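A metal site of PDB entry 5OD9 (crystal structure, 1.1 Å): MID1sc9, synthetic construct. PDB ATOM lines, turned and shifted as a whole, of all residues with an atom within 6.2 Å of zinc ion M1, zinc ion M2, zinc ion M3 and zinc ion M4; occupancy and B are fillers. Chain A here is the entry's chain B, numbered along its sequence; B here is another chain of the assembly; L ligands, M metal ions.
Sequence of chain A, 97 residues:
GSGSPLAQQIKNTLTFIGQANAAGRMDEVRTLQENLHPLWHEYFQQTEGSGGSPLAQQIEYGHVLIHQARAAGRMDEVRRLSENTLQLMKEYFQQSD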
ATOM      1  N   GLN A  33      30.795  13.585  13.294  1.00  0.00           N
ATOM      2  CA  GLN A  33      30.041  12.365  13.370  1.00  0.00           C
ATOM      3  C   GLN A  33      28.901  12.367  12.375  1.00  0.00           C
ATOM      4  O   GLN A  33      28.546  11.372  11.748  1.00  0.00           O
ATOM      5  CB  GLN A  33      29.448  12.239  14.786  1.00  0.00           C
ATOM      6  CG  GLN A  33      30.492  11.817  15.815  1.00  0.00           C
ATOM      7  CD  GLN A  33      29.970  11.782  17.242  1.00  0.00           C
ATOM      8  OE1 GLN A  33      28.820  12.202  17.516  1.00  0.00           O
ATOM      9  NE2 GLN A  33      30.862  11.263  18.088  1.00  0.00           N
ATOM     10  N   GLU A  34      28.280  13.537  12.219  1.00  0.00           N
ATOM     11  CA  GLU A  34      27.183  13.717  11.252  1.00  0.00           C
ATOM     12  C   GLU A  34      27.691  13.761   9.829  1.00  0.00           C
ATOM     13  O   GLU A  34      27.038  13.207   8.957  1.00  0.00           O
ATOM     14  CB  GLU A  34      26.320  14.906  11.639  1.00  0.00           C
ATOM     15  CG  GLU A  34      25.284  14.475  12.664  1.00  0.00           C
ATOM     16  CD  GLU A  34      24.117  13.771  12.030  1.00  0.00           C
ATOM     17  OE1 GLU A  34      24.321  12.584  11.622  1.00  0.00           O
ATOM     18  OE2 GLU A  34      23.074  14.443  11.890  1.00  0.00           O
ATOM     19  N   HIS A  37      27.929  10.147   8.611  1.00  0.00           N
ATOM     20  CA  HIS A  37      26.720   9.402   8.267  1.00  0.00           C
ATOM     21  C   HIS A  37      26.548   9.316   6.775  1.00  0.00           C
ATOM     22  O   HIS A  37      26.501   8.164   6.290  1.00  0.00           O
ATOM     23  CB  HIS A  37      25.621  10.048   9.130  1.00  0.00           C
ATOM     24  CG  HIS A  37      24.240   9.573   8.862  1.00  0.00           C
ATOM     25  ND1 HIS A  37      23.193  10.148   9.508  1.00  0.00           N
ATOM     26  CD2 HIS A  37      23.714   8.620   8.067  1.00  0.00           C
ATOM     27  CE1 HIS A  37      22.097   9.508   9.083  1.00  0.00           C
ATOM     28  NE2 HIS A  37      22.367   8.578   8.182  1.00  0.00           N
ATOM     29  N   PRO A  38      26.326  10.384   6.025  1.00  0.00           N
ATOM     30  CA  PRO A  38      26.184  10.162   4.576  1.00  0.00           C
ATOM     31  C   PRO A  38      27.413   9.524   3.952  1.00  0.00           C
ATOM     32  O   PRO A  38      27.288   8.806   2.980  1.00  0.00           O
ATOM     33  CB  PRO A  38      25.930  11.538   3.977  1.00  0.00           C
ATOM     34  CG  PRO A  38      25.750  12.467   5.114  1.00  0.00           C
ATOM     35  CD  PRO A  38      26.117  11.772   6.370  1.00  0.00           C
ATOM     36  N   HIS A  41      27.094   5.841   4.276  1.00  0.00           N
ATOM     37  CA  HIS A  41      26.138   5.271   3.345  1.00  0.00           C
ATOM     38  C   HIS A  41      26.696   5.181   1.934  1.00  0.00           C
ATOM     39  O   HIS A  41      26.432   4.195   1.252  1.00  0.00           O
ATOM     40  CB  HIS A  41      24.859   6.111   3.289  1.00  0.00           C
ATOM     41  CG  HIS A  41      23.922   6.035   4.420  1.00  0.00           C
ATOM     42  ND1 HIS A  41      23.640   4.917   5.172  1.00  0.00           N
ATOM     43  CD2 HIS A  41      23.113   6.996   4.950  1.00  0.00           C
ATOM     44  CE1 HIS A  41      22.734   5.180   6.046  1.00  0.00           C
ATOM     45  NE2 HIS A  41      22.365   6.457   5.949  1.00  0.00           N
ATOM     46  N   HIS A  63      23.413   3.818  11.681  1.00  0.00           N
ATOM     47  CA  HIS A  63      23.030   5.123  11.130  1.00  0.00           C
ATOM     48  C   HIS A  63      21.540   5.264  10.915  1.00  0.00           C
ATOM     49  O   HIS A  63      20.989   6.311  11.241  1.00  0.00           O
ATOM     50  CB  HIS A  63      23.791   5.401   9.848  1.00  0.00           C
ATOM     51  CG  HIS A  63      25.244   5.644  10.116  1.00  0.00           C
ATOM     52  ND1 HIS A  63      25.754   6.772  10.653  1.00  0.00           N
ATOM     53  CD2 HIS A  63      26.263   4.791   9.923  1.00  0.00           C
ATOM     54  CE1 HIS A  63      27.078   6.649  10.782  1.00  0.00           C
ATOM     55  NE2 HIS A  63      27.445   5.436  10.350  1.00  0.00           N
ATOM     56  N   VAL A  64      20.882   4.247  10.405  1.00  0.00           N
ATOM     57  CA  VAL A  64      19.410   4.258  10.251  1.00  0.00           C
ATOM     58  C   VAL A  64      18.744   4.580  11.586  1.00  0.00           C
ATOM     59  O   VAL A  64      17.836   5.394  11.672  1.00  0.00           O
ATOM     60  CB  VAL A  64      18.878   2.948   9.623  1.00  0.00           C
ATOM     61  CG1 VAL A  64      17.377   2.880   9.712  1.00  0.00           C
ATOM     62  CG2 VAL A  64      19.374   2.775   8.210  1.00  0.00           C
ATOM     63  N   ILE A  66      20.147   5.872  14.409  1.00  0.00           N
ATOM     64  CA  ILE A  66      20.494   7.233  14.873  1.00  0.00           C
ATOM     65  C   ILE A  66      19.525   8.221  14.245  1.00  0.00           C
ATOM     66  O   ILE A  66      19.004   9.098  14.931  1.00  0.00           O
ATOM     67  CB  ILE A  66      21.915   7.578  14.575  1.00  0.00           C
ATOM     68  CG1 ILE A  66      22.930   6.728  15.368  1.00  0.00           C
ATOM     69  CG2 ILE A  66      22.183   9.061  14.785  1.00  0.00           C
ATOM     70  CD1 ILE A  66      24.297   6.694  14.790  1.00  0.00           C
ATOM     71  N   HIS A  67      19.302   8.098  12.935  1.00  0.00           N
ATOM     72  CA  HIS A  67      18.459   9.066  12.260  1.00  0.00           C
ATOM     73  C   HIS A  67      17.015   9.024  12.795  1.00  0.00           C
ATOM     74  O   HIS A  67      16.404  10.074  13.051  1.00  0.00           O
ATOM     75  CB  HIS A  67      18.498   8.800  10.744  1.00  0.00           C
ATOM     76  CG  HIS A  67      18.043   9.991   9.942  1.00  0.00           C
ATOM     77  ND1 HIS A  67      18.169  10.037   8.573  1.00  0.00           N
ATOM     78  CD2 HIS A  67      17.557  11.189  10.279  1.00  0.00           C
ATOM     79  CE1 HIS A  67      17.763  11.210   8.134  1.00  0.00           C
ATOM     80  NE2 HIS A  67      17.397  11.950   9.153  1.00  0.00           N
ATOM     81  N   ARG A  70      16.901  10.653  16.144  1.00  0.00           N
ATOM     82  CA  ARG A  70      16.964  12.097  16.084  1.00  0.00           C
ATOM     83  C   ARG A  70      15.642  12.720  15.654  1.00  0.00           C
ATOM     84  O   ARG A  70      15.195  13.706  16.169  1.00  0.00           O
ATOM     85  CB  ARG A  70      18.151  12.500  15.182  1.00  0.00           C
ATOM     86  CG  ARG A  70      18.580  13.927  15.465  1.00  0.00           C
ATOM     87  CD  ARG A  70      19.623  14.391  14.446  1.00  0.00           C
ATOM     88  NE  ARG A  70      20.718  13.446  14.270  1.00  0.00           N
ATOM     89  CZ  ARG A  70      21.848  13.404  14.963  1.00  0.00           C
ATOM     90  NH1 ARG A  70      22.080  14.248  15.912  1.00  0.00           N
ATOM     91  NH2 ARG A  70      22.725  12.460  14.632  1.00  0.00           N
ATOM     92  N   ALA A  71      14.988  12.059  14.690  1.00  0.00           N
ATOM     93  CA  ALA A  71      13.720  12.573  14.167  1.00  0.00           C
ATOM     94  C   ALA A  71      12.658  12.577  15.277  1.00  0.00           C
ATOM     95  O   ALA A  71      11.769  13.408  15.253  1.00  0.00           O
ATOM     96  CB  ALA A  71      13.225  11.726  12.988  1.00  0.00           C
ATOM     97  N   GLN B  33      22.352  17.854  -0.423  1.00  0.00           N
ATOM     98  CA  GLN B  33      21.641  17.353   0.769  1.00  0.00           C
ATOM     99  C   GLN B  33      22.619  16.915   1.864  1.00  0.00           C
ATOM    100  O   GLN B  33      22.408  17.184   3.048  1.00  0.00           O
ATOM    101  CB  GLN B  33      20.723  16.243   0.353  1.00  0.00           C
ATOM    102  CG  GLN B  33      19.497  16.726  -0.479  1.00  0.00           C
ATOM    103  CD  GLN B  33      18.600  15.590  -0.913  1.00  0.00           C
ATOM    104  OE1 GLN B  33      19.100  14.473  -1.130  1.00  0.00           O
ATOM    105  NE2 GLN B  33      17.334  15.842  -1.145  1.00  0.00           N
ATOM    106  N   GLU B  34      23.675  16.224   1.453  1.00  0.00           N
ATOM    107  CA  GLU B  34      24.600  15.698   2.447  1.00  0.00           C
ATOM    108  C   GLU B  34      25.372  16.820   3.118  1.00  0.00           C
ATOM    109  O   GLU B  34      25.682  16.710   4.315  1.00  0.00           O
ATOM    110  CB  GLU B  34      25.508  14.665   1.744  1.00  0.00           C
ATOM    111  CG  GLU B  34      24.683  13.428   1.378  1.00  0.00           C
ATOM    112  CD  GLU B  34      25.434  12.370   0.613  1.00  0.00           C
ATOM    113  OE1 GLU B  34      26.501  12.645   0.090  1.00  0.00           O
ATOM    114  OE2 GLU B  34      24.844  11.279   0.546  1.00  0.00           O
ATOM    115  N   HIS B  37      22.837  18.056   5.685  1.00  0.00           N
ATOM    116  CA  HIS B  37      22.460  17.089   6.752  1.00  0.00           C
ATOM    117  C   HIS B  37      22.843  17.505   8.163  1.00  0.00           C
ATOM    118  O   HIS B  37      21.926  17.595   9.013  1.00  0.00           O
ATOM    119  CB  HIS B  37      22.991  15.710   6.336  1.00  0.00           C
ATOM    120  CG  HIS B  37      22.677  14.581   7.237  1.00  0.00           C
ATOM    121  ND1 HIS B  37      21.752  13.595   6.902  1.00  0.00           N
ATOM    122  CD2 HIS B  37      23.141  14.258   8.484  1.00  0.00           C
ATOM    123  CE1 HIS B  37      21.732  12.757   7.921  1.00  0.00           C
ATOM    124  NE2 HIS B  37      22.541  13.103   8.932  1.00  0.00           N
ATOM    125  N   TRP B  40      20.862  20.979   9.074  1.00  0.00           N
ATOM    126  CA  TRP B  40      19.446  20.768   9.337  1.00  0.00           C
ATOM    127  C   TRP B  40      19.217  20.013  10.629  1.00  0.00           C
ATOM    128  O   TRP B  40      18.331  20.368  11.411  1.00  0.00           O
ATOM    129  CB  TRP B  40      18.814  20.006   8.155  1.00  0.00           C
ATOM    130  CG  TRP B  40      17.453  19.509   8.489  1.00  0.00           C
ATOM    131  CD1 TRP B  40      17.100  18.182   8.615  1.00  0.00           C
ATOM    132  CD2 TRP B  40      16.261  20.242   8.748  1.00  0.00           C
ATOM    133  NE1 TRP B  40      15.789  18.061   8.941  1.00  0.00           N
ATOM    134  CE2 TRP B  40      15.242  19.317   9.029  1.00  0.00           C
ATOM    135  CE3 TRP B  40      15.935  21.635   8.781  1.00  0.00           C
ATOM    136  CZ2 TRP B  40      13.956  19.701   9.331  1.00  0.00           C
ATOM    137  CZ3 TRP B  40      14.654  22.006   9.079  1.00  0.00           C
ATOM    138  CH2 TRP B  40      13.706  21.044   9.348  1.00  0.00           C
ATOM    139  N   HIS B  41      20.014  19.003  10.926  1.00  0.00           N
ATOM    140  CA  HIS B  41      19.788  18.312  12.196  1.00  0.00           C
ATOM    141  C   HIS B  41      20.095  19.165  13.406  1.00  0.00           C
ATOM    142  O   HIS B  41      19.350  19.132  14.377  1.00  0.00           O
ATOM    143  CB  HIS B  41      20.606  17.025  12.197  1.00  0.00           C
ATOM    144  CG  HIS B  41      19.875  15.947  11.442  1.00  0.00           C
ATOM    145  ND1 HIS B  41      20.480  14.753  11.102  1.00  0.00           N
ATOM    146  CD2 HIS B  41      18.591  15.870  11.003  1.00  0.00           C
ATOM    147  CE1 HIS B  41      19.578  14.021  10.463  1.00  0.00           C
ATOM    148  NE2 HIS B  41      18.424  14.625  10.362  1.00  0.00           N
ATOM    149  N   GLU B  60      11.249  16.500   8.412  1.00  0.00           N
ATOM    150  CA  GLU B  60      12.261  15.575   8.923  1.00  0.00           C
ATOM    151  C   GLU B  60      11.937  14.129   8.590  1.00  0.00           C
ATOM    152  O   GLU B  60      12.832  13.340   8.248  1.00  0.00           O
ATOM    153  CB  GLU B  60      12.480  15.829  10.425  1.00  0.00           C
ATOM    154  CG  GLU B  60      13.371  14.823  11.084  1.00  0.00           C
ATOM    155  CD  GLU B  60      14.744  14.572  10.440  1.00  0.00           C
ATOM    156  OE1 GLU B  60      15.251  15.440   9.748  1.00  0.00           O
ATOM    157  OE2 GLU B  60      15.277  13.475  10.597  1.00  0.00           O
ATOM    158  N   HIS B  63      13.153  13.558   5.169  1.00  0.00           N
ATOM    159  CA  HIS B  63      14.569  13.338   5.194  1.00  0.00           C
ATOM    160  C   HIS B  63      14.928  11.894   5.562  1.00  0.00           C
ATOM    161  O   HIS B  63      15.751  11.301   4.895  1.00  0.00           O
ATOM    162  CB  HIS B  63      15.182  14.342   6.208  1.00  0.00           C
ATOM    163  CG  HIS B  63      16.694  14.273   6.216  1.00  0.00           C
ATOM    164  ND1 HIS B  63      17.376  14.441   7.449  1.00  0.00           N
ATOM    165  CD2 HIS B  63      17.610  14.123   5.250  1.00  0.00           C
ATOM    166  CE1 HIS B  63      18.670  14.377   7.104  1.00  0.00           C
ATOM    167  NE2 HIS B  63      18.882  14.191   5.806  1.00  0.00           N
ATOM    168  N   VAL B  64      14.292  11.379   6.592  1.00  0.00           N
ATOM    169  CA  VAL B  64      14.505   9.966   6.939  1.00  0.00           C
ATOM    170  C   VAL B  64      14.172   9.098   5.744  1.00  0.00           C
ATOM    171  O   VAL B  64      14.955   8.147   5.433  1.00  0.00           O
ATOM    172  CB  VAL B  64      13.608   9.612   8.145  1.00  0.00           C
ATOM    173  CG1 VAL B  64      13.542   8.120   8.356  1.00  0.00           C
ATOM    174  CG2 VAL B  64      14.089  10.330   9.413  1.00  0.00           C
ATOM    175  N   HIS B  67      16.789   9.125   2.977  1.00  0.00           N
ATOM    176  CA  HIS B  67      17.881   8.237   3.241  1.00  0.00           C
ATOM    177  C   HIS B  67      17.516   6.807   2.904  1.00  0.00           C
ATOM    178  O   HIS B  67      18.288   6.066   2.306  1.00  0.00           O
ATOM    179  CB  HIS B  67      18.316   8.297   4.715  1.00  0.00           C
ATOM    180  CG  HIS B  67      19.250   9.385   5.044  1.00  0.00           C
ATOM    181  ND1 HIS B  67      20.476   9.196   5.672  1.00  0.00           N
ATOM    182  CD2 HIS B  67      19.173  10.700   4.763  1.00  0.00           C
ATOM    183  CE1 HIS B  67      21.056  10.386   5.765  1.00  0.00           C
ATOM    184  NE2 HIS B  67      20.312  11.347   5.227  1.00  0.00           N
ATOM    185  N   GLN B  68      16.314   6.395   3.233  1.00  0.00           N
ATOM    186  CA  GLN B  68      15.911   5.011   2.978  1.00  0.00           C
ATOM    187  C   GLN B  68      15.770   4.733   1.480  1.00  0.00           C
ATOM    188  O   GLN B  68      16.198   3.698   1.022  1.00  0.00           O
ATOM    189  CB  GLN B  68      14.625   4.639   3.719  1.00  0.00           C
ATOM    190  CG  GLN B  68      14.890   4.668   5.235  1.00  0.00           C
ATOM    191  CD  GLN B  68      15.497   3.465   5.900  1.00  0.00           C
ATOM    192  OE1 GLN B  68      15.126   2.309   5.679  1.00  0.00           O
ATOM    193  NE2 GLN B  68      16.468   3.633   6.807  1.00  0.00           N
ATOM    194  N   ARG B  70      17.302   6.363  -0.944  1.00  0.00           N
ATOM    195  CA  ARG B  70      18.639   6.417  -1.562  1.00  0.00           C
ATOM    196  C   ARG B  70      19.329   5.083  -1.272  1.00  0.00           C
ATOM    197  O   ARG B  70      19.971   4.566  -2.209  1.00  0.00           O
ATOM    198  CB  ARG B  70      19.415   7.658  -1.070  1.00  0.00           C
ATOM    199  CG  ARG B  70      20.900   7.748  -1.255  1.00  0.00           C
ATOM    200  CD  ARG B  70      21.348   9.224  -1.030  1.00  0.00           C
ATOM    201  NE  ARG B  70      20.791  10.184  -1.980  1.00  0.00           N
ATOM    202  CZ  ARG B  70      20.231  11.341  -1.715  1.00  0.00           C
ATOM    203  NH1 ARG B  70      20.148  11.751  -0.444  1.00  0.00           N
ATOM    204  NH2 ARG B  70      19.741  12.121  -2.718  1.00  0.00           N
HETATM  205 CL1  LIG L   1      19.233   6.907   7.779  1.00  0.00          CL
HETATM  206 CL1  LG2 L   2      21.432  13.982   3.303  1.00  0.00          CL
HETATM  207 CL1  LG3 L   3      21.116  11.328  11.754  1.00  0.00          CL
HETATM  208 ZN    ZN M   1      21.097   7.710   6.893  1.00  0.00          ZN
HETATM  209 ZN    ZN M   2      20.626  13.342   5.264  1.00  0.00          ZN
HETATM  210 ZN    ZN M   3      22.904  11.888  10.478  1.00  0.00          ZN
HETATM  211 ZN    ZN M   4      16.865  13.939   9.300  1.00  0.00          ZN
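A ring nitrogen (ND1) of His 41 of chain B lies within hydrogen-bond range of the side-chain carboxylate of Glu 34 of chain A. The guanidinium group of Arg 70 of chain A lies within salt-bridge range of the side-chain carboxylate of Glu 34 of chain A, at 3.4 Å. A ring nitrogen (NE2) of His 37 of chain B sits close to a ring nitrogen (ND1) of His 41 of chain B, 3.4 Å away. A ring nitrogen (ND1) of His 41 of chain B is in hydrogen-bond range of the guanidinium group (NE) of Arg 70 of chain A. NE1 of Trp 40 of chain B sits close to OE1 of Glu 60 of chain B, at 2.8 Å.
Three residues have an atom within 4 Å of zinc ion M1: His 37 of chain A, His 41 of chain A and His 67 of chain B.
Three residues have an atom within 4 Å of zinc ion M2: His 37 of chain B, His 63 of chain B and His 67 of chain B. The nearest printed residue that does not touch zinc ion M2 is His 67 of chain A (4.6 Å).
Of the 22 residues printed, 4 come within 4 Å of zinc ion M3.
Within 4 Å of zinc ion M4: His 67 of chain A, His 41 of chain B, Glu 60 of chain B and His 63 of chain B.
Zinc ion M1 is bound by NE2 of His 37 of chain A, NE2 of His 41 of chain A, ND1 of His 67 of chain B and CL1 of LIG L1.
Zinc ion M2 is bound by ND1 of His 37 of chain B, NE2 of His 63 of chain B, NE2 of His 67 of chain B and CL1 of LG2 L2. Zinc ion M2 has four donor atoms within binding distance.
Zinc ion M3 is bound by the side-chain carboxylate (OE1) of Glu 34 of chain A (1.9 Å), a ring nitrogen (NE2) of His 37 of chain B (2.0 Å), a ring nitrogen (ND1) of His 37 of chain A (2.0 Å) and a chlorine (CL1) of LG3 L3 (2.3 Å).
Zinc ion M4 is bound by ND1 of His 63 of chain B (2.0 Å), NE2 of His 41 of chain B (2.0 Å), NE2 of His 67 of chain A (2.1 Å), OE2 of Glu 60 of chain B (2.1 Å) and OE1 of Glu 60 of chain B (2.2 Å). Zinc ion M4 has five donor atoms within binding distance.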
